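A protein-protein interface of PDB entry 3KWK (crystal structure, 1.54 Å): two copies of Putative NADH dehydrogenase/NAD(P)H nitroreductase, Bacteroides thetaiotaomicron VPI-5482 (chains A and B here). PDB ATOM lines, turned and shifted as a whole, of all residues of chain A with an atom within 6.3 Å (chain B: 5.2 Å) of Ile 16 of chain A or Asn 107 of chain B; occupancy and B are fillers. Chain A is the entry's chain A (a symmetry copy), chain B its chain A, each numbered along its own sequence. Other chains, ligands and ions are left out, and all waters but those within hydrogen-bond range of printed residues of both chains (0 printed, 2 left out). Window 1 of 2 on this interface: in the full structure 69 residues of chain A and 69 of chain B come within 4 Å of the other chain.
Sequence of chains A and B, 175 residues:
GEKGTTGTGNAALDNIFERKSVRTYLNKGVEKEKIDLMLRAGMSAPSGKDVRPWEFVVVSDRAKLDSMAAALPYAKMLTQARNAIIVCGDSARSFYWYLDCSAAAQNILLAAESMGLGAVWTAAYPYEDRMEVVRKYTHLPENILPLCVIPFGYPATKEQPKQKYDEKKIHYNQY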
ATOM      1  N   ALA A  11      18.435   1.178  16.169  1.00  0.00           N
ATOM      2  CA  ALA A  11      18.507   1.701  14.787  1.00  0.00           C
ATOM      3  C   ALA A  11      19.336   0.814  13.867  1.00  0.00           C
ATOM      4  O   ALA A  11      19.064   0.734  12.656  1.00  0.00           O
ATOM      5  CB  ALA A  11      19.049   3.183  14.756  1.00  0.00           C
ATOM      6  N   ALA A  12      20.371   0.153  14.382  1.00  0.00           N
ATOM      7  CA  ALA A  12      21.155  -0.760  13.544  1.00  0.00           C
ATOM      8  C   ALA A  12      20.289  -1.931  13.035  1.00  0.00           C
ATOM      9  O   ALA A  12      20.323  -2.323  11.852  1.00  0.00           O
ATOM     10  CB  ALA A  12      22.412  -1.288  14.280  1.00  0.00           C
ATOM     11  N   LEU A  13      19.548  -2.550  13.952  1.00  0.00           N
ATOM     12  CA  LEU A  13      18.634  -3.618  13.574  1.00  0.00           C
ATOM     13  C   LEU A  13      17.572  -3.098  12.635  1.00  0.00           C
ATOM     14  O   LEU A  13      17.324  -3.746  11.646  1.00  0.00           O
ATOM     15  CB  LEU A  13      17.966  -4.234  14.809  1.00  0.00           C
ATOM     16  CG  LEU A  13      18.835  -5.114  15.688  1.00  0.00           C
ATOM     17  CD1 LEU A  13      17.995  -5.470  16.963  1.00  0.00           C
ATOM     18  CD2 LEU A  13      19.289  -6.349  14.926  1.00  0.00           C
ATOM     19  N   ASP A  14      17.009  -1.903  12.878  1.00  0.00           N
ATOM     20  CA  ASP A  14      16.004  -1.358  11.957  1.00  0.00           C
ATOM     21  C   ASP A  14      16.542  -1.271  10.554  1.00  0.00           C
ATOM     22  O   ASP A  14      15.854  -1.594   9.579  1.00  0.00           O
ATOM     23  CB  ASP A  14      15.546   0.016  12.420  1.00  0.00           C
ATOM     24  CG  ASP A  14      14.653  -0.040  13.688  1.00  0.00           C
ATOM     25  OD1 ASP A  14      14.157  -1.122  14.048  1.00  0.00           O
ATOM     26  OD2 ASP A  14      14.518   1.018  14.316  1.00  0.00           O
ATOM     27  N   ASN A  15      17.784  -0.822  10.424  1.00  0.00           N
ATOM     28  CA  ASN A  15      18.410  -0.651   9.086  1.00  0.00           C
ATOM     29  C   ASN A  15      18.610  -2.014   8.404  1.00  0.00           C
ATOM     30  O   ASN A  15      18.388  -2.178   7.218  1.00  0.00           O
ATOM     31  CB  ASN A  15      19.721   0.124   9.250  1.00  0.00           C
ATOM     32  CG  ASN A  15      20.548   0.216   7.966  1.00  0.00           C
ATOM     33  OD1 ASN A  15      21.570  -0.434   7.865  1.00  0.00           O
ATOM     34  ND2 ASN A  15      20.085   1.008   7.037  1.00  0.00           N
ATOM     35  N   ILE A  16      19.054  -3.008   9.177  1.00  0.00           N
ATOM     36  CA  ILE A  16      19.186  -4.351   8.657  1.00  0.00           C
ATOM     37  C   ILE A  16      17.824  -4.880   8.140  1.00  0.00           C
ATOM     38  O   ILE A  16      17.734  -5.524   7.080  1.00  0.00           O
ATOM     39  CB  ILE A  16      19.758  -5.302   9.738  1.00  0.00           C
ATOM     40  CG1 ILE A  16      21.260  -5.042   9.937  1.00  0.00           C
ATOM     41  CG2 ILE A  16      19.493  -6.791   9.386  1.00  0.00           C
ATOM     42  CD1 ILE A  16      21.879  -5.605  11.262  1.00  0.00           C
ATOM     43  N   PHE A  17      16.768  -4.616   8.904  1.00  0.00           N
ATOM     44  CA  PHE A  17      15.425  -5.080   8.520  1.00  0.00           C
ATOM     45  C   PHE A  17      14.822  -4.295   7.345  1.00  0.00           C
ATOM     46  O   PHE A  17      14.035  -4.854   6.576  1.00  0.00           O
ATOM     47  CB  PHE A  17      14.468  -5.031   9.713  1.00  0.00           C
ATOM     48  CG  PHE A  17      14.897  -5.874  10.905  1.00  0.00           C
ATOM     49  CD1 PHE A  17      15.642  -7.026  10.775  1.00  0.00           C
ATOM     50  CD2 PHE A  17      14.541  -5.474  12.181  1.00  0.00           C
ATOM     51  CE1 PHE A  17      16.017  -7.766  11.928  1.00  0.00           C
ATOM     52  CE2 PHE A  17      14.896  -6.207  13.301  1.00  0.00           C
ATOM     53  CZ  PHE A  17      15.666  -7.356  13.154  1.00  0.00           C
ATOM     54  N   GLU A  18      15.250  -3.050   7.172  1.00  0.00           N
ATOM     55  CA  GLU A  18      14.692  -2.143   6.176  1.00  0.00           C
ATOM     56  C   GLU A  18      15.356  -2.289   4.813  1.00  0.00           C
ATOM     57  O   GLU A  18      14.757  -1.995   3.768  1.00  0.00           O
ATOM     58  CB  GLU A  18      14.854  -0.702   6.645  1.00  0.00           C
ATOM     59  CG  GLU A  18      14.352   0.363   5.690  1.00  0.00           C
ATOM     60  CD  GLU A  18      12.877   0.225   5.315  1.00  0.00           C
ATOM     61  OE1 GLU A  18      12.065  -0.236   6.158  1.00  0.00           O
ATOM     62  OE2 GLU A  18      12.556   0.613   4.163  1.00  0.00           O
ATOM     63  N   ARG A  19      16.599  -2.752   4.804  1.00  0.00           N
ATOM     64  CA  ARG A  19      17.341  -2.841   3.570  1.00  0.00           C
ATOM     65  C   ARG A  19      16.587  -3.698   2.532  1.00  0.00           C
ATOM     66  O   ARG A  19      16.018  -4.752   2.857  1.00  0.00           O
ATOM     67  CB  ARG A  19      18.733  -3.449   3.814  1.00  0.00           C
ATOM     68  CG  ARG A  19      19.625  -3.606   2.612  1.00  0.00           C
ATOM     69  CD  ARG A  19      20.518  -4.859   2.602  1.00  0.00           C
ATOM     70  NE  ARG A  19      19.686  -6.065   2.727  1.00  0.00           N
ATOM     71  CZ  ARG A  19      18.963  -6.603   1.737  1.00  0.00           C
ATOM     72  NH1 ARG A  19      19.067  -6.158   0.481  1.00  0.00           N
ATOM     73  NH2 ARG A  19      18.167  -7.629   2.008  1.00  0.00           N
ATOM     74  N   GLN A 106      27.789  -6.447   1.913  1.00  0.00           N
ATOM     75  CA  GLN A 106      26.589  -6.300   2.736  1.00  0.00           C
ATOM     76  C   GLN A 106      26.703  -5.008   3.551  1.00  0.00           C
ATOM     77  O   GLN A 106      25.717  -4.264   3.714  1.00  0.00           O
ATOM     78  CB  GLN A 106      26.388  -7.483   3.700  1.00  0.00           C
ATOM     79  CG  GLN A 106      25.209  -7.356   4.671  1.00  0.00           C
ATOM     80  CD  GLN A 106      23.868  -7.228   4.015  1.00  0.00           C
ATOM     81  OE1 GLN A 106      23.756  -7.311   2.772  1.00  0.00           O
ATOM     82  NE2 GLN A 106      22.818  -7.056   4.830  1.00  0.00           N
ATOM     83  N   LEU A 110      24.002  -1.916   3.436  1.00  0.00           N
ATOM     84  CA  LEU A 110      23.436  -1.400   4.674  1.00  0.00           C
ATOM     85  C   LEU A 110      23.707   0.101   4.791  1.00  0.00           C
ATOM     86  O   LEU A 110      22.812   0.905   5.125  1.00  0.00           O
ATOM     87  CB  LEU A 110      23.932  -2.187   5.876  1.00  0.00           C
ATOM     88  CG  LEU A 110      23.429  -3.593   6.016  1.00  0.00           C
ATOM     89  CD1 LEU A 110      24.165  -4.289   7.189  1.00  0.00           C
ATOM     90  CD2 LEU A 110      21.963  -3.586   6.272  1.00  0.00           C
ATOM     91  N   ALA B  41      17.959 -10.961  12.088  1.00  0.00           N
ATOM     92  CA  ALA B  41      18.904 -10.186  11.343  1.00  0.00           C
ATOM     93  C   ALA B  41      19.573 -11.026  10.212  1.00  0.00           C
ATOM     94  O   ALA B  41      19.637 -10.615   9.037  1.00  0.00           O
ATOM     95  CB  ALA B  41      20.003  -9.541  12.262  1.00  0.00           C
ATOM     96  N   GLY B  42      20.030 -12.222  10.586  1.00  0.00           N
ATOM     97  CA  GLY B  42      20.611 -13.150   9.611  1.00  0.00           C
ATOM     98  C   GLY B  42      19.682 -13.421   8.431  1.00  0.00           C
ATOM     99  O   GLY B  42      20.123 -13.379   7.273  1.00  0.00           O
ATOM    100  N   SER B  44      17.506 -11.554   7.170  1.00  0.00           N
ATOM    101  CA  SER B  44      17.208 -10.311   6.397  1.00  0.00           C
ATOM    102  C   SER B  44      18.253 -10.045   5.334  1.00  0.00           C
ATOM    103  O   SER B  44      18.112  -9.086   4.582  1.00  0.00           O
ATOM    104  CB  SER B  44      17.161  -9.118   7.337  1.00  0.00           C
ATOM    105  OG  SER B  44      16.178  -9.338   8.350  1.00  0.00           O
ATOM    106  N   ALA B  45      19.265 -10.897   5.249  1.00  0.00           N
ATOM    107  CA  ALA B  45      20.280 -10.768   4.196  1.00  0.00           C
ATOM    108  C   ALA B  45      19.708 -10.770   2.761  1.00  0.00           C
ATOM    109  O   ALA B  45      18.632 -11.336   2.466  1.00  0.00           O
ATOM    110  CB  ALA B  45      21.299 -11.936   4.308  1.00  0.00           C
ATOM    111  N   SER B 102      27.324 -15.579   3.894  1.00  0.00           N
ATOM    112  CA  SER B 102      28.304 -14.585   4.399  1.00  0.00           C
ATOM    113  C   SER B 102      27.608 -13.259   4.708  1.00  0.00           C
ATOM    114  O   SER B 102      27.919 -12.608   5.722  1.00  0.00           O
ATOM    115  CB  SER B 102      29.349 -14.345   3.318  1.00  0.00           C
ATOM    116  OG  SER B 102      30.222 -15.455   3.214  1.00  0.00           O
ATOM    117  N   ALA B 103      26.663 -12.847   3.855  1.00  0.00           N
ATOM    118  CA  ALA B 103      25.890 -11.639   4.152  1.00  0.00           C
ATOM    119  C   ALA B 103      25.023 -11.847   5.437  1.00  0.00           C
ATOM    120  O   ALA B 103      24.937 -10.961   6.272  1.00  0.00           O
ATOM    121  CB  ALA B 103      25.017 -11.225   2.925  1.00  0.00           C
ATOM    122  N   ALA B 104      24.460 -13.053   5.584  1.00  0.00           N
ATOM    123  CA  ALA B 104      23.654 -13.400   6.766  1.00  0.00           C
ATOM    124  C   ALA B 104      24.543 -13.360   8.005  1.00  0.00           C
ATOM    125  O   ALA B 104      24.161 -12.814   9.053  1.00  0.00           O
ATOM    126  CB  ALA B 104      22.986 -14.789   6.641  1.00  0.00           C
ATOM    127  N   ALA B 105      25.733 -13.940   7.886  1.00  0.00           N
ATOM    128  CA  ALA B 105      26.635 -13.955   9.015  1.00  0.00           C
ATOM    129  C   ALA B 105      27.017 -12.542   9.424  1.00  0.00           C
ATOM    130  O   ALA B 105      27.094 -12.255  10.617  1.00  0.00           O
ATOM    131  CB  ALA B 105      27.890 -14.782   8.681  1.00  0.00           C
ATOM    132  N   GLN B 106      27.243 -11.666   8.451  1.00  0.00           N
ATOM    133  CA  GLN B 106      27.651 -10.298   8.770  1.00  0.00           C
ATOM    134  C   GLN B 106      26.489  -9.585   9.469  1.00  0.00           C
ATOM    135  O   GLN B 106      26.690  -8.829  10.438  1.00  0.00           O
ATOM    136  CB  GLN B 106      28.051  -9.496   7.520  1.00  0.00           C
ATOM    137  CG  GLN B 106      28.392  -8.021   7.758  1.00  0.00           C
ATOM    138  CD  GLN B 106      29.544  -7.787   8.687  1.00  0.00           C
ATOM    139  OE1 GLN B 106      30.202  -8.748   9.142  1.00  0.00           O
ATOM    140  NE2 GLN B 106      29.837  -6.509   8.966  1.00  0.00           N
ATOM    141  N   ASN B 107      25.245  -9.801   9.028  1.00  0.00           N
ATOM    142  CA  ASN B 107      24.092  -9.266   9.775  1.00  0.00           C
ATOM    143  C   ASN B 107      24.048  -9.753  11.226  1.00  0.00           C
ATOM    144  O   ASN B 107      23.709  -8.990  12.123  1.00  0.00           O
ATOM    145  CB  ASN B 107      22.796  -9.624   9.085  1.00  0.00           C
ATOM    146  CG  ASN B 107      22.474  -8.709   7.931  1.00  0.00           C
ATOM    147  OD1 ASN B 107      23.187  -7.725   7.653  1.00  0.00           O
ATOM    148  ND2 ASN B 107      21.355  -9.019   7.246  1.00  0.00           N
ATOM    149  N   ILE B 108      24.355 -11.020  11.441  1.00  0.00           N
ATOM    150  CA  ILE B 108      24.368 -11.571  12.802  1.00  0.00           C
ATOM    151  C   ILE B 108      25.425 -10.873  13.631  1.00  0.00           C
ATOM    152  O   ILE B 108      25.192 -10.500  14.813  1.00  0.00           O
ATOM    153  CB  ILE B 108      24.597 -13.106  12.794  1.00  0.00           C
ATOM    154  CG1 ILE B 108      23.329 -13.788  12.192  1.00  0.00           C
ATOM    155  CG2 ILE B 108      24.956 -13.642  14.230  1.00  0.00           C
ATOM    156  CD1 ILE B 108      23.431 -15.252  11.869  1.00  0.00           C
ATOM    157  N   LEU B 109      26.616 -10.706  13.054  1.00  0.00           N
ATOM    158  CA  LEU B 109      27.697 -10.007  13.804  1.00  0.00           C
ATOM    159  C   LEU B 109      27.331  -8.562  14.138  1.00  0.00           C
ATOM    160  O   LEU B 109      27.549  -8.103  15.265  1.00  0.00           O
ATOM    161  CB  LEU B 109      28.984 -10.020  12.982  1.00  0.00           C
ATOM    162  CG  LEU B 109      29.614 -11.384  12.645  1.00  0.00           C
ATOM    163  CD1 LEU B 109      30.905 -11.195  11.739  1.00  0.00           C
ATOM    164  CD2 LEU B 109      29.937 -12.196  13.914  1.00  0.00           C
ATOM    165  N   LEU B 110      26.684  -7.884  13.201  1.00  0.00           N
ATOM    166  CA  LEU B 110      26.260  -6.504  13.393  1.00  0.00           C
ATOM    167  C   LEU B 110      25.167  -6.434  14.463  1.00  0.00           C
ATOM    168  O   LEU B 110      25.198  -5.584  15.377  1.00  0.00           O
ATOM    169  CB  LEU B 110      25.842  -5.869  12.077  1.00  0.00           C
ATOM    170  CG  LEU B 110      26.934  -5.588  11.088  1.00  0.00           C
ATOM    171  CD1 LEU B 110      26.309  -5.104   9.754  1.00  0.00           C
ATOM    172  CD2 LEU B 110      27.851  -4.546  11.624  1.00  0.00           C
ATOM    173  N   ALA B 111      24.216  -7.366  14.405  1.00  0.00           N
ATOM    174  CA  ALA B 111      23.155  -7.451  15.382  1.00  0.00           C
ATOM    175  C   ALA B 111      23.711  -7.649  16.790  1.00  0.00           C
ATOM    176  O   ALA B 111      23.317  -6.950  17.738  1.00  0.00           O
ATOM    177  CB  ALA B 111      22.160  -8.624  14.986  1.00  0.00           C
ATOM    178  N   ALA B 112      24.640  -8.594  16.929  1.00  0.00           N
ATOM    179  CA  ALA B 112      25.310  -8.848  18.203  1.00  0.00           C
ATOM    180  C   ALA B 112      25.933  -7.558  18.769  1.00  0.00           C
ATOM    181  O   ALA B 112      25.669  -7.182  19.909  1.00  0.00           O
ATOM    182  CB  ALA B 112      26.353  -9.979  18.046  1.00  0.00           C
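Leu 110 of chain B touches its own counterpart, Leu 110 of chain A.
Positions printed for both chains: 106 and 110.
Of the 12 pairs that touch across the chains among the printed residues, 1 has its exchanged pair printed and touching as well.
Ile 16 of chain A touches just these residues of chain B: Ala 41 (3.8 Å), Ser 44 (3.6 Å) and Asn 107 (3.6 Å).
Asn 107 of chain B touches three residues of chain A.
Of the printed residues of chain B, Arg 19 of chain A touches Ser 44 and Ala 45.
Printed residues of chain B within 4 Å of Leu 110 of chain A: Asn 107 and Leu 110.
Of the printed residues of chain A, Ala 111 of chain B touches Leu 13.
Printed residues of chain B within 4 Å of Phe 17 of chain A: Ala 41 (3.7 Å) and Ser 44 (3.4 Å).
Of the printed residues of chain A, Ala 41 of chain B touches Ile 16 (3.8 Å) and Phe 17 (3.7 Å).
The side-chain amide oxygen (OD1) of Asn 107 of chain B is in hydrogen-bond range of the side-chain amide nitrogen (NE2) of Gln 106 of chain A, 2.9 Å away.
The backbone carbonyl oxygen (O) of Ser 44 of chain B sits at hydrogen-bond distance from the guanidinium group (NH2) of Arg 19 of chain A (3.0 Å).
CB of Ala 111 of chain B touches CD2 of Leu 13 of chain A, 3.7 Å away.
Ala 41 of chain B touches Ile 16 of chain A.
Ile 16 of chain A touches Ser 44 of chain B (O to CB, 3.6 Å).
CG2 of Ile 16 of chain A touches ND2 of Asn 107 of chain B, at 3.6 Å.
Phe 17 of chain A touches Ala 41 of chain B.
Phe 17 of chain A touches Ser 44 of chain B (CD1 to OG, 3.4 Å).
Arg 19 of chain A touches Ala 45 of chain B (NH2 to C, 3.6 Å).
CG of Gln 106 of chain A touches O of Ala 103 of chain B, 3.95 Å away.
Leu 110 of chain A touches Asn 107 of chain B (CD1 to OD1, 3.6 Å).
Leu 110 of chain B touches Leu 110 of chain A.
Hydrophobic or aromatic side chains of chain A that line the printed part of chain B: Leu 13, Ile 16, Phe 17 and Leu 110.
Of the 15 printed residues of chain B, 7 touch a printed residue of chain A.
Hydrophobic or aromatic side chains of chain B that line the printed part of chain A: Leu 110 and Ala 111.
Among the printed residues, no Asp or Glu carboxylate lies within 4 Å of a Lys or Arg side-chain nitrogen of the other chain.
The side-chain amide oxygen (OD1) of Asn 15 of chain A lies close to the backbone carbonyl oxygen (O) of Leu 110 of chain A, 3.3 Å away.
The backbone carbonyl oxygen of Ala 41 of chain B sits at hydrogen-bond distance from the side-chain amide nitrogen of Asn 107 of chain B, at 3.0 Å.
ND2 of Asn 107 of chain B sits close to N of Ala 45 of chain B, 3.4 Å away.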
